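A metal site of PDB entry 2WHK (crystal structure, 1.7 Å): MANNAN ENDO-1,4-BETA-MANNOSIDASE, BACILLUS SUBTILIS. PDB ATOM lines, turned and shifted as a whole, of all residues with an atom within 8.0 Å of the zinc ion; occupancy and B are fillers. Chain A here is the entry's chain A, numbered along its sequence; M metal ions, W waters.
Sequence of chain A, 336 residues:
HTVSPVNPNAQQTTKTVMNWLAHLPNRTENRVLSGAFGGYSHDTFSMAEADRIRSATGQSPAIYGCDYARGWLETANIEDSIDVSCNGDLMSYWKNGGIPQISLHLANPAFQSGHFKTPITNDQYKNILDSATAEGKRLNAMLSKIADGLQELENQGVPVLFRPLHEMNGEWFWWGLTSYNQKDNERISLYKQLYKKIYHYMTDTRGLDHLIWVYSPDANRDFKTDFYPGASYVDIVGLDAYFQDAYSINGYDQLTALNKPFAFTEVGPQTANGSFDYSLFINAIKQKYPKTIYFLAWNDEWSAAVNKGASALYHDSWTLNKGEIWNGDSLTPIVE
NE2 of His 23 binds the zinc ion, at 2.2 Å. N of His 1 is bound to the zinc ion, 2.2 Å away. The zinc ion is bound by water W1 (2.3 Å). The side-chain carboxylate (OE1) of Glu 336 is bound to the zinc ion. A ring nitrogen (ND1) of His 1 binds the zinc ion. O of His 1 binds the zinc ion, 2.3 Å away. The zinc ion has six donor atoms within binding distance.
ND1 of His 23 lies within hydrogen-bond range of O of Asn 19 (2.7 Å).
The nearest printed residue that does not touch the zinc ion is Thr 2 (4.3 Å).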
ATOM      1  N   HIS A   1      23.629   5.794  -8.251  1.00  0.00           N
ATOM      2  CA  HIS A   1      22.303   5.419  -7.682  1.00  0.00           C
ATOM      3  C   HIS A   1      22.511   4.707  -6.344  1.00  0.00           C
ATOM      4  O   HIS A   1      23.638   4.374  -5.979  1.00  0.00           O
ATOM      5  CB  HIS A   1      21.531   4.524  -8.651  1.00  0.00           C
ATOM      6  CG  HIS A   1      22.044   3.119  -8.728  1.00  0.00           C
ATOM      7  ND1 HIS A   1      23.390   2.806  -8.681  1.00  0.00           N
ATOM      8  CD2 HIS A   1      21.391   1.936  -8.865  1.00  0.00           C
ATOM      9  CE1 HIS A   1      23.534   1.497  -8.791  1.00  0.00           C
ATOM     10  NE2 HIS A   1      22.339   0.949  -8.907  1.00  0.00           N
ATOM     11  N   THR A   2      21.401   4.483  -5.636  1.00  0.00           N
ATOM     12  CA  THR A   2      21.427   3.763  -4.373  1.00  0.00           C
ATOM     13  C   THR A   2      20.663   2.431  -4.478  1.00  0.00           C
ATOM     14  O   THR A   2      19.478   2.415  -4.858  1.00  0.00           O
ATOM     15  CB  THR A   2      20.813   4.599  -3.247  1.00  0.00           C
ATOM     16  OG1 THR A   2      21.628   5.749  -3.015  1.00  0.00           O
ATOM     17  CG2 THR A   2      20.697   3.781  -1.951  1.00  0.00           C
ATOM     18  N   VAL A   3      21.332   1.340  -4.146  1.00  0.00           N
ATOM     19  CA  VAL A   3      20.657   0.040  -4.063  1.00  0.00           C
ATOM     20  C   VAL A   3      20.301  -0.208  -2.607  1.00  0.00           C
ATOM     21  O   VAL A   3      21.190  -0.275  -1.753  1.00  0.00           O
ATOM     22  CB  VAL A   3      21.521  -1.093  -4.598  1.00  0.00           C
ATOM     23  CG1 VAL A   3      20.849  -2.454  -4.353  1.00  0.00           C
ATOM     24  CG2 VAL A   3      21.791  -0.877  -6.076  1.00  0.00           C
ATOM     25  N   ASN A  19      24.274  -1.508  -0.385  1.00  0.00           N
ATOM     26  CA  ASN A  19      24.592  -0.561  -1.448  1.00  0.00           C
ATOM     27  C   ASN A  19      26.031  -0.690  -1.918  1.00  0.00           C
ATOM     28  O   ASN A  19      26.322  -0.679  -3.122  1.00  0.00           O
ATOM     29  CB  ASN A  19      24.334   0.869  -0.981  1.00  0.00           C
ATOM     30  CG  ASN A  19      24.525   1.866  -2.090  1.00  0.00           C
ATOM     31  OD1 ASN A  19      23.810   1.828  -3.085  1.00  0.00           O
ATOM     32  ND2 ASN A  19      25.472   2.781  -1.908  1.00  0.00           N
ATOM     33  N   ALA A  22      26.578  -3.752  -4.104  1.00  0.00           N
ATOM     34  CA  ALA A  22      26.012  -3.568  -5.446  1.00  0.00           C
ATOM     35  C   ALA A  22      26.923  -2.767  -6.381  1.00  0.00           C
ATOM     36  O   ALA A  22      26.851  -2.948  -7.610  1.00  0.00           O
ATOM     37  CB  ALA A  22      24.632  -2.930  -5.352  1.00  0.00           C
ATOM     38  N   HIS A  23      27.762  -1.893  -5.819  1.00  0.00           N
ATOM     39  CA  HIS A  23      28.674  -1.058  -6.616  1.00  0.00           C
ATOM     40  C   HIS A  23      30.066  -1.650  -6.847  1.00  0.00           C
ATOM     41  O   HIS A  23      30.887  -1.024  -7.501  1.00  0.00           O
ATOM     42  CB  HIS A  23      28.813   0.333  -5.971  1.00  0.00           C
ATOM     43  CG  HIS A  23      27.585   1.162  -6.097  1.00  0.00           C
ATOM     44  ND1 HIS A  23      26.479   0.988  -5.289  1.00  0.00           N
ATOM     45  CD2 HIS A  23      27.282   2.185  -6.938  1.00  0.00           C
ATOM     46  CE1 HIS A  23      25.550   1.867  -5.633  1.00  0.00           C
ATOM     47  NE2 HIS A  23      26.010   2.599  -6.635  1.00  0.00           N
ATOM     48  N   ASN A  26      31.884  -1.775 -10.377  1.00  0.00           N
ATOM     49  CA  ASN A  26      32.403  -0.510 -10.934  1.00  0.00           C
ATOM     50  C   ASN A  26      33.892  -0.279 -10.671  1.00  0.00           C
ATOM     51  O   ASN A  26      34.488   0.642 -11.242  1.00  0.00           O
ATOM     52  CB  ASN A  26      31.601   0.677 -10.419  1.00  0.00           C
ATOM     53  CG  ASN A  26      30.135   0.610 -10.786  1.00  0.00           C
ATOM     54  OD1 ASN A  26      29.740  -0.091 -11.720  1.00  0.00           O
ATOM     55  ND2 ASN A  26      29.316   1.355 -10.051  1.00  0.00           N
ATOM     56  N   ILE A 334      32.671   3.892  -2.279  1.00  0.00           N
ATOM     57  CA  ILE A 334      31.900   3.439  -3.417  1.00  0.00           C
ATOM     58  C   ILE A 334      32.421   4.128  -4.680  1.00  0.00           C
ATOM     59  O   ILE A 334      32.683   5.337  -4.686  1.00  0.00           O
ATOM     60  CB  ILE A 334      30.413   3.774  -3.233  1.00  0.00           C
ATOM     61  CG1 ILE A 334      29.798   2.851  -2.177  1.00  0.00           C
ATOM     62  CG2 ILE A 334      29.652   3.635  -4.529  1.00  0.00           C
ATOM     63  CD1 ILE A 334      28.481   3.326  -1.678  1.00  0.00           C
ATOM     64  N   VAL A 335      32.585   3.341  -5.735  1.00  0.00           N
ATOM     65  CA  VAL A 335      32.739   3.903  -7.086  1.00  0.00           C
ATOM     66  C   VAL A 335      31.358   3.904  -7.739  1.00  0.00           C
ATOM     67  O   VAL A 335      30.760   2.836  -7.943  1.00  0.00           O
ATOM     68  CB  VAL A 335      33.750   3.108  -7.944  1.00  0.00           C
ATOM     69  CG1 VAL A 335      33.793   3.678  -9.372  1.00  0.00           C
ATOM     70  CG2 VAL A 335      35.134   3.141  -7.305  1.00  0.00           C
ATOM     71  N   GLU A 336      30.851   5.097  -8.043  1.00  0.00           N
ATOM     72  CA  GLU A 336      29.518   5.267  -8.628  1.00  0.00           C
ATOM     73  C   GLU A 336      29.550   4.984 -10.123  1.00  0.00           C
ATOM     74  O   GLU A 336      28.503   4.784 -10.736  1.00  0.00           O
ATOM     75  CB  GLU A 336      29.007   6.696  -8.391  1.00  0.00           C
ATOM     76  CG  GLU A 336      28.633   6.973  -6.939  1.00  0.00           C
ATOM     77  CD  GLU A 336      27.392   6.231  -6.480  1.00  0.00           C
ATOM     78  OE1 GLU A 336      26.570   5.807  -7.346  1.00  0.00           O
ATOM     79  OE2 GLU A 336      27.218   6.064  -5.248  1.00  0.00           O
ATOM     80  OXT GLU A 336      30.606   4.968 -10.742  1.00  0.00           O
HETATM   81 ZN    ZN M   1      25.083   4.170  -7.815  1.00  0.00          ZN
HETATM   82  O   HOH W   1      26.247   3.918  -9.729  1.00  0.00           O
